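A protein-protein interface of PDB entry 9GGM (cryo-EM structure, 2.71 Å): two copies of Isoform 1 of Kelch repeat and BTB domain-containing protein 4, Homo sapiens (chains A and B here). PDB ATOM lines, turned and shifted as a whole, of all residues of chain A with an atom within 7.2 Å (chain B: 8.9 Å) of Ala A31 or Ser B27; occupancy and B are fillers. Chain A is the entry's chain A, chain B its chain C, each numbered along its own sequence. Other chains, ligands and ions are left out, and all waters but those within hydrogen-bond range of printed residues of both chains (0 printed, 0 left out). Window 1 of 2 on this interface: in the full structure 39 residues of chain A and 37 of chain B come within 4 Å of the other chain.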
ATOM      1  N   SER A  25       6.437   9.995   4.547  1.00  0.00           N
ATOM      2  CA  SER A  25       5.653  11.191   4.815  1.00  0.00           C
ATOM      3  C   SER A  25       4.559  11.426   3.779  1.00  0.00           C
ATOM      4  O   SER A  25       3.898  12.467   3.822  1.00  0.00           O
ATOM      5  CB  SER A  25       6.567  12.415   4.894  1.00  0.00           C
ATOM      6  OG  SER A  25       7.796  12.094   5.519  1.00  0.00           O
ATOM      7  N   HIS A  26       4.362  10.493   2.843  1.00  0.00           N
ATOM      8  CA  HIS A  26       3.311  10.658   1.844  1.00  0.00           C
ATOM      9  C   HIS A  26       1.938  10.741   2.499  1.00  0.00           C
ATOM     10  O   HIS A  26       1.130  11.620   2.170  1.00  0.00           O
ATOM     11  CB  HIS A  26       3.358   9.508   0.838  1.00  0.00           C
ATOM     12  CG  HIS A  26       2.062   9.282   0.124  1.00  0.00           C
ATOM     13  ND1 HIS A  26       1.525  10.202  -0.751  1.00  0.00           N
ATOM     14  CD2 HIS A  26       1.192   8.245   0.159  1.00  0.00           C
ATOM     15  CE1 HIS A  26       0.385   9.741  -1.228  1.00  0.00           C
ATOM     16  NE2 HIS A  26       0.158   8.555  -0.692  1.00  0.00           N
ATOM     17  N   SER A  27       1.655   9.824   3.428  1.00  0.00           N
ATOM     18  CA  SER A  27       0.356   9.816   4.093  1.00  0.00           C
ATOM     19  C   SER A  27       0.133  11.097   4.885  1.00  0.00           C
ATOM     20  O   SER A  27      -0.953  11.685   4.833  1.00  0.00           O
ATOM     21  CB  SER A  27       0.239   8.593   5.003  1.00  0.00           C
ATOM     22  OG  SER A  27       1.234   8.608   6.012  1.00  0.00           O
ATOM     23  N   GLY A  28       1.150  11.546   5.623  1.00  0.00           N
ATOM     24  CA  GLY A  28       1.009  12.782   6.377  1.00  0.00           C
ATOM     25  C   GLY A  28       0.743  13.976   5.482  1.00  0.00           C
ATOM     26  O   GLY A  28      -0.146  14.790   5.755  1.00  0.00           O
ATOM     27  N   ARG A  29       1.512  14.095   4.396  1.00  0.00           N
ATOM     28  CA  ARG A  29       1.334  15.219   3.480  1.00  0.00           C
ATOM     29  C   ARG A  29      -0.058  15.206   2.864  1.00  0.00           C
ATOM     30  O   ARG A  29      -0.740  16.237   2.823  1.00  0.00           O
ATOM     31  CB  ARG A  29       2.402  15.189   2.384  1.00  0.00           C
ATOM     32  CG  ARG A  29       3.793  15.606   2.832  1.00  0.00           C
ATOM     33  CD  ARG A  29       4.694  15.863   1.632  1.00  0.00           C
ATOM     34  NE  ARG A  29       4.778  14.708   0.746  1.00  0.00           N
ATOM     35  CZ  ARG A  29       5.656  13.723   0.877  1.00  0.00           C
ATOM     36  NH1 ARG A  29       6.551  13.719   1.851  1.00  0.00           N
ATOM     37  NH2 ARG A  29       5.637  12.718   0.007  1.00  0.00           N
ATOM     38  N   VAL A  30      -0.498  14.042   2.377  1.00  0.00           N
ATOM     39  CA  VAL A  30      -1.798  13.978   1.715  1.00  0.00           C
ATOM     40  C   VAL A  30      -2.920  14.255   2.711  1.00  0.00           C
ATOM     41  O   VAL A  30      -3.891  14.947   2.386  1.00  0.00           O
ATOM     42  CB  VAL A  30      -1.985  12.634   0.980  1.00  0.00           C
ATOM     43  CG1 VAL A  30      -2.054  11.464   1.945  1.00  0.00           C
ATOM     44  CG2 VAL A  30      -3.229  12.681   0.103  1.00  0.00           C
ATOM     45  N   ALA A  31      -2.805  13.737   3.940  1.00  0.00           N
ATOM     46  CA  ALA A  31      -3.838  13.976   4.943  1.00  0.00           C
ATOM     47  C   ALA A  31      -3.916  15.453   5.308  1.00  0.00           C
ATOM     48  O   ALA A  31      -5.007  16.034   5.380  1.00  0.00           O
ATOM     49  CB  ALA A  31      -3.568  13.126   6.185  1.00  0.00           C
ATOM     50  N   GLN A  32      -2.763  16.084   5.542  1.00  0.00           N
ATOM     51  CA  GLN A  32      -2.771  17.500   5.884  1.00  0.00           C
ATOM     52  C   GLN A  32      -3.344  18.332   4.744  1.00  0.00           C
ATOM     53  O   GLN A  32      -4.142  19.250   4.974  1.00  0.00           O
ATOM     54  CB  GLN A  32      -1.357  17.965   6.234  1.00  0.00           C
ATOM     55  N   GLY A  33      -2.946  18.028   3.506  1.00  0.00           N
ATOM     56  CA  GLY A  33      -3.470  18.774   2.375  1.00  0.00           C
ATOM     57  C   GLY A  33      -4.962  18.601   2.163  1.00  0.00           C
ATOM     58  O   GLY A  33      -5.668  19.572   1.882  1.00  0.00           O
ATOM     59  N   ILE A  34      -5.471  17.371   2.297  1.00  0.00           N
ATOM     60  CA  ILE A  34      -6.914  17.177   2.152  1.00  0.00           C
ATOM     61  C   ILE A  34      -7.652  17.939   3.246  1.00  0.00           C
ATOM     62  O   ILE A  34      -8.650  18.618   2.982  1.00  0.00           O
ATOM     63  CB  ILE A  34      -7.295  15.680   2.087  1.00  0.00           C
ATOM     64  CG1 ILE A  34      -6.848  14.846   3.293  1.00  0.00           C
ATOM     65  CG2 ILE A  34      -6.765  15.056   0.800  1.00  0.00           C
ATOM     66  CD1 ILE A  34      -7.803  14.848   4.482  1.00  0.00           C
ATOM     67  N   MET A  35      -7.172  17.837   4.491  1.00  0.00           N
ATOM     68  CA  MET A  35      -7.773  18.597   5.582  1.00  0.00           C
ATOM     69  C   MET A  35      -7.844  20.080   5.236  1.00  0.00           C
ATOM     70  O   MET A  35      -8.916  20.695   5.294  1.00  0.00           O
ATOM     71  CB  MET A  35      -6.977  18.380   6.870  1.00  0.00           C
ATOM     72  CG  MET A  35      -7.179  19.464   7.918  1.00  0.00           C
ATOM     73  SD  MET A  35      -6.133  19.261   9.375  1.00  0.00           S
ATOM     74  CE  MET A  35      -5.688  17.530   9.252  1.00  0.00           C
ATOM     75  N   LYS A  36      -6.704  20.664   4.854  1.00  0.00           N
ATOM     76  CA  LYS A  36      -6.648  22.100   4.600  1.00  0.00           C
ATOM     77  C   LYS A  36      -7.582  22.496   3.462  1.00  0.00           C
ATOM     78  O   LYS A  36      -8.413  23.400   3.612  1.00  0.00           O
ATOM     79  CB  LYS A  36      -5.212  22.522   4.293  1.00  0.00           C
ATOM     80  N   LEU A  37      -7.464  21.829   2.311  1.00  0.00           N
ATOM     81  CA  LEU A  37      -8.264  22.237   1.160  1.00  0.00           C
ATOM     82  C   LEU A  37      -9.752  22.031   1.412  1.00  0.00           C
ATOM     83  O   LEU A  37     -10.562  22.900   1.075  1.00  0.00           O
ATOM     84  CB  LEU A  37      -7.814  21.507  -0.107  1.00  0.00           C
ATOM     85  CG  LEU A  37      -6.612  22.108  -0.847  1.00  0.00           C
ATOM     86  CD1 LEU A  37      -5.272  21.623  -0.323  1.00  0.00           C
ATOM     87  CD2 LEU A  37      -6.733  21.835  -2.341  1.00  0.00           C
ATOM     88  N   GLN A  66     -12.629   6.067   5.058  1.00  0.00           N
ATOM     89  CA  GLN A  66     -12.763   5.731   6.468  1.00  0.00           C
ATOM     90  C   GLN A  66     -13.949   4.831   6.768  1.00  0.00           C
ATOM     91  O   GLN A  66     -13.869   4.011   7.684  1.00  0.00           O
ATOM     92  CB  GLN A  66     -12.904   7.009   7.311  1.00  0.00           C
ATOM     93  CG  GLN A  66     -11.688   7.915   7.308  1.00  0.00           C
ATOM     94  CD  GLN A  66     -10.923   7.853   8.613  1.00  0.00           C
ATOM     95  OE1 GLN A  66     -10.397   6.808   8.989  1.00  0.00           O
ATOM     96  NE2 GLN A  66     -10.867   8.977   9.317  1.00  0.00           N
ATOM     97  N   TYR A 104     -12.955  14.243   8.391  1.00  0.00           N
ATOM     98  CA  TYR A 104     -11.912  15.051   7.770  1.00  0.00           C
ATOM     99  C   TYR A 104     -10.721  15.300   8.692  1.00  0.00           C
ATOM    100  O   TYR A 104      -9.572  15.101   8.286  1.00  0.00           O
ATOM    101  CB  TYR A 104     -12.500  16.387   7.308  1.00  0.00           C
ATOM    102  CG  TYR A 104     -13.471  16.264   6.158  1.00  0.00           C
ATOM    103  CD1 TYR A 104     -13.021  16.055   4.862  1.00  0.00           C
ATOM    104  CD2 TYR A 104     -14.839  16.358   6.368  1.00  0.00           C
ATOM    105  CE1 TYR A 104     -13.906  15.942   3.807  1.00  0.00           C
ATOM    106  CE2 TYR A 104     -15.732  16.247   5.320  1.00  0.00           C
ATOM    107  CZ  TYR A 104     -15.261  16.039   4.042  1.00  0.00           C
ATOM    108  OH  TYR A 104     -16.146  15.929   2.996  1.00  0.00           O
ATOM    109  N   ASP B  23      -6.900  10.277  16.805  1.00  0.00           N
ATOM    110  CA  ASP B  23      -6.748   8.998  16.122  1.00  0.00           C
ATOM    111  C   ASP B  23      -5.463   9.009  15.302  1.00  0.00           C
ATOM    112  O   ASP B  23      -5.395   9.641  14.243  1.00  0.00           O
ATOM    113  CB  ASP B  23      -7.963   8.741  15.235  1.00  0.00           C
ATOM    114  CG  ASP B  23      -8.506  10.016  14.605  1.00  0.00           C
ATOM    115  OD1 ASP B  23      -7.708  10.900  14.230  1.00  0.00           O
ATOM    116  OD2 ASP B  23      -9.737  10.144  14.486  1.00  0.00           O
ATOM    117  N   ARG B  24      -4.442   8.303  15.789  1.00  0.00           N
ATOM    118  CA  ARG B  24      -3.165   8.274  15.086  1.00  0.00           C
ATOM    119  C   ARG B  24      -3.244   7.555  13.746  1.00  0.00           C
ATOM    120  O   ARG B  24      -2.327   7.702  12.930  1.00  0.00           O
ATOM    121  CB  ARG B  24      -2.101   7.614  15.965  1.00  0.00           C
ATOM    122  N   SER B  25      -4.304   6.787  13.500  1.00  0.00           N
ATOM    123  CA  SER B  25      -4.455   6.017  12.273  1.00  0.00           C
ATOM    124  C   SER B  25      -5.350   6.700  11.247  1.00  0.00           C
ATOM    125  O   SER B  25      -5.651   6.099  10.211  1.00  0.00           O
ATOM    126  CB  SER B  25      -4.995   4.622  12.593  1.00  0.00           C
ATOM    127  OG  SER B  25      -4.109   3.915  13.444  1.00  0.00           O
ATOM    128  N   HIS B  26      -5.792   7.931  11.513  1.00  0.00           N
ATOM    129  CA  HIS B  26      -6.636   8.637  10.554  1.00  0.00           C
ATOM    130  C   HIS B  26      -5.911   8.850   9.230  1.00  0.00           C
ATOM    131  O   HIS B  26      -6.465   8.589   8.155  1.00  0.00           O
ATOM    132  CB  HIS B  26      -7.090   9.973  11.142  1.00  0.00           C
ATOM    133  CG  HIS B  26      -7.489  10.983  10.111  1.00  0.00           C
ATOM    134  ND1 HIS B  26      -8.589  10.819   9.298  1.00  0.00           N
ATOM    135  CD2 HIS B  26      -6.937  12.169   9.762  1.00  0.00           C
ATOM    136  CE1 HIS B  26      -8.698  11.860   8.492  1.00  0.00           C
ATOM    137  NE2 HIS B  26      -7.708  12.694   8.753  1.00  0.00           N
ATOM    138  N   SER B  27      -4.663   9.324   9.291  1.00  0.00           N
ATOM    139  CA  SER B  27      -3.905   9.575   8.071  1.00  0.00           C
ATOM    140  C   SER B  27      -3.672   8.289   7.288  1.00  0.00           C
ATOM    141  O   SER B  27      -3.829   8.264   6.063  1.00  0.00           O
ATOM    142  CB  SER B  27      -2.574  10.245   8.410  1.00  0.00           C
ATOM    143  OG  SER B  27      -1.783   9.416   9.243  1.00  0.00           O
ATOM    144  N   GLY B  28      -3.305   7.209   7.980  1.00  0.00           N
ATOM    145  CA  GLY B  28      -3.100   5.943   7.294  1.00  0.00           C
ATOM    146  C   GLY B  28      -4.362   5.444   6.617  1.00  0.00           C
ATOM    147  O   GLY B  28      -4.336   5.025   5.455  1.00  0.00           O
ATOM    148  N   ARG B  29      -5.487   5.488   7.337  1.00  0.00           N
ATOM    149  CA  ARG B  29      -6.748   5.021   6.772  1.00  0.00           C
ATOM    150  C   ARG B  29      -7.141   5.846   5.553  1.00  0.00           C
ATOM    151  O   ARG B  29      -7.517   5.294   4.512  1.00  0.00           O
ATOM    152  CB  ARG B  29      -7.856   5.068   7.827  1.00  0.00           C
ATOM    153  CG  ARG B  29      -7.775   3.978   8.886  1.00  0.00           C
ATOM    154  CD  ARG B  29      -9.071   3.896   9.683  1.00  0.00           C
ATOM    155  NE  ARG B  29      -9.425   5.166  10.305  1.00  0.00           N
ATOM    156  CZ  ARG B  29      -9.012   5.557  11.503  1.00  0.00           C
ATOM    157  NH1 ARG B  29      -8.224   4.797  12.245  1.00  0.00           N
ATOM    158  NH2 ARG B  29      -9.402   6.739  11.970  1.00  0.00           N
ATOM    159  N   VAL B  30      -7.063   7.175   5.664  1.00  0.00           N
ATOM    160  CA  VAL B  30      -7.485   8.022   4.553  1.00  0.00           C
ATOM    161  C   VAL B  30      -6.564   7.830   3.353  1.00  0.00           C
ATOM    162  O   VAL B  30      -7.026   7.787   2.207  1.00  0.00           O
ATOM    163  CB  VAL B  30      -7.588   9.500   4.984  1.00  0.00           C
ATOM    164  CG1 VAL B  30      -6.232  10.084   5.340  1.00  0.00           C
ATOM    165  CG2 VAL B  30      -8.258  10.323   3.892  1.00  0.00           C
ATOM    166  N   ALA B  31      -5.253   7.699   3.588  1.00  0.00           N
ATOM    167  CA  ALA B  31      -4.319   7.500   2.485  1.00  0.00           C
ATOM    168  C   ALA B  31      -4.577   6.172   1.783  1.00  0.00           C
ATOM    169  O   ALA B  31      -4.615   6.103   0.548  1.00  0.00           O
ATOM    170  CB  ALA B  31      -2.881   7.572   2.996  1.00  0.00           C
ATOM    171  N   GLN B  32      -4.754   5.099   2.557  1.00  0.00           N
ATOM    172  CA  GLN B  32      -5.016   3.802   1.946  1.00  0.00           C
ATOM    173  C   GLN B  32      -6.319   3.823   1.159  1.00  0.00           C
ATOM    174  O   GLN B  32      -6.388   3.294   0.042  1.00  0.00           O
ATOM    175  CB  GLN B  32      -5.049   2.714   3.018  1.00  0.00           C
ATOM    176  N   GLY B  33      -7.367   4.427   1.726  1.00  0.00           N
ATOM    177  CA  GLY B  33      -8.633   4.494   1.018  1.00  0.00           C
ATOM    178  C   GLY B  33      -8.579   5.318  -0.255  1.00  0.00           C
ATOM    179  O   GLY B  33      -9.142   4.921  -1.278  1.00  0.00           O
ATOM    180  N   ILE B  34      -7.903   6.471  -0.222  1.00  0.00           N
ATOM    181  CA  ILE B  34      -7.785   7.264  -1.445  1.00  0.00           C
ATOM    182  C   ILE B  34      -7.011   6.483  -2.499  1.00  0.00           C
ATOM    183  O   ILE B  34      -7.406   6.435  -3.668  1.00  0.00           O
ATOM    184  CB  ILE B  34      -7.193   8.666  -1.169  1.00  0.00           C
ATOM    185  CG1 ILE B  34      -5.806   8.653  -0.515  1.00  0.00           C
ATOM    186  CG2 ILE B  34      -8.160   9.494  -0.328  1.00  0.00           C
ATOM    187  CD1 ILE B  34      -4.632   8.603  -1.484  1.00  0.00           C
ATOM    188  N   MET B  35      -5.896   5.860  -2.100  1.00  0.00           N
ATOM    189  CA  MET B  35      -5.141   5.024  -3.028  1.00  0.00           C
ATOM    190  C   MET B  35      -6.044   3.984  -3.681  1.00  0.00           C
ATOM    191  O   MET B  35      -6.111   3.884  -4.912  1.00  0.00           O
ATOM    192  CB  MET B  35      -3.979   4.348  -2.297  1.00  0.00           C
ATOM    193  CG  MET B  35      -3.434   3.116  -3.003  1.00  0.00           C
ATOM    194  SD  MET B  35      -2.108   2.291  -2.096  1.00  0.00           S
ATOM    195  CE  MET B  35      -1.594   3.583  -0.967  1.00  0.00           C
ATOM    196  N   LEU B  61      -7.565  16.513  -5.329  1.00  0.00           N
ATOM    197  CA  LEU B  61      -7.185  16.649  -3.927  1.00  0.00           C
ATOM    198  C   LEU B  61      -5.859  15.955  -3.639  1.00  0.00           C
ATOM    199  O   LEU B  61      -5.027  16.480  -2.890  1.00  0.00           O
ATOM    200  CB  LEU B  61      -8.290  16.092  -3.029  1.00  0.00           C
ATOM    201  N   VAL B  62      -5.650  14.771  -4.218  1.00  0.00           N
ATOM    202  CA  VAL B  62      -4.434  14.007  -3.945  1.00  0.00           C
ATOM    203  C   VAL B  62      -3.202  14.776  -4.410  1.00  0.00           C
ATOM    204  O   VAL B  62      -2.193  14.858  -3.698  1.00  0.00           O
ATOM    205  CB  VAL B  62      -4.514  12.618  -4.603  1.00  0.00           C
ATOM    206  N   ALA B  65      -2.667  18.153  -2.468  1.00  0.00           N
ATOM    207  CA  ALA B  65      -2.171  17.939  -1.115  1.00  0.00           C
ATOM    208  C   ALA B  65      -0.677  17.657  -1.066  1.00  0.00           C
ATOM    209  O   ALA B  65      -0.105  17.619   0.029  1.00  0.00           O
ATOM    210  CB  ALA B  65      -2.926  16.779  -0.460  1.00  0.00           C
ATOM    211  N   GLN B  66      -0.037  17.460  -2.214  1.00  0.00           N
ATOM    212  CA  GLN B  66       1.395  17.211  -2.291  1.00  0.00           C
ATOM    213  C   GLN B  66       2.161  18.297  -3.025  1.00  0.00           C
ATOM    214  O   GLN B  66       3.314  18.563  -2.679  1.00  0.00           O
ATOM    215  CB  GLN B  66       1.669  15.871  -2.993  1.00  0.00           C
ATOM    216  CG  GLN B  66       1.170  14.646  -2.251  1.00  0.00           C
ATOM    217  CD  GLN B  66       2.298  13.862  -1.613  1.00  0.00           C
ATOM    218  OE1 GLN B  66       2.999  14.362  -0.735  1.00  0.00           O
ATOM    219  NE2 GLN B  66       2.490  12.629  -2.065  1.00  0.00           N
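The side-chain amide nitrogen (NE2) of Gln B66 sits at hydrogen-bond distance from a ring nitrogen (ND1) of His A26, 2.9 Å away. The side-chain amide oxygen of Gln B66 sits close to the guanidinium group of Arg A29 (3.2 Å). The side-chain amide nitrogen of Gln A66 sits at hydrogen-bond distance from a ring nitrogen (ND1) of His B26. OE1 of Gln A66 sits close to NH2 of Arg B29 (3.1 Å). O of Tyr A104 is in hydrogen-bond range of NE2 of His B26 (3.1 Å). The backbone carbonyl oxygen (O) of Arg A29 lies close to the backbone carbonyl oxygen (O) of Ala B65.
Among the printed residues, merely in contact across the chains: Gly A33 with Ala B65, Val A30 with Ala B65, Ala A31 with Ser B27, Ile A34 with Ala B65 and Ser A27 with Ala B31.
Of chain B, only Ser B27 (3.8 Å) comes within 4 Å of Ala A31. Ser B27 touches just one residue of chain A: Ala A31 (3.8 Å). No residue of chain B comes within 4 Å of Gly A28. Val A30 touches just one residue of chain B: Ala B65 (3.5 Å). Of the printed residues of chain B, Tyr A104 touches His B26. Of the printed residues of chain B, Arg A29 touches Ala B65 (3.2 Å) and Gln B66 (2.3 Å). Printed residues of chain A within 4 Å of His B26: Gln A66 and Tyr A104. Printed residues of chain B within 4 Å of Gln A66: His B26 (2.9 Å) and Arg B29 (2.3 Å). Ser B25 touches none of the printed residues of chain A. Gly B33 touches none of the printed residues of chain A. The nearest residue of chain B that does not touch Ala A31 is Val B30 (4.1 Å).
Printed residues of chain B that touch a printed residue of chain A: His B26, Ser B27, Arg B29, Ala B31, Ala B65 and Gln B66. Hydrophobic or aromatic side chains of chain A that line the printed part of chain B: His A26 and Ala A31. Among the printed residues, no Asp or Glu carboxylate lies within 4 Å of a Lys or Arg side-chain nitrogen of the other chain.
His A26 touches Gln B66, and with the chains exchanged Gln A66 touches His B26. Ser A27 touches Ala B31, and with the chains exchanged Ala A31 touches Ser B27. Arg A29 touches Gln B66, and with the chains exchanged Gln A66 touches Arg B29. Of the 11 pairs that touch across the chains among the printed residues, 6 have their exchanged pair printed and touching as well.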
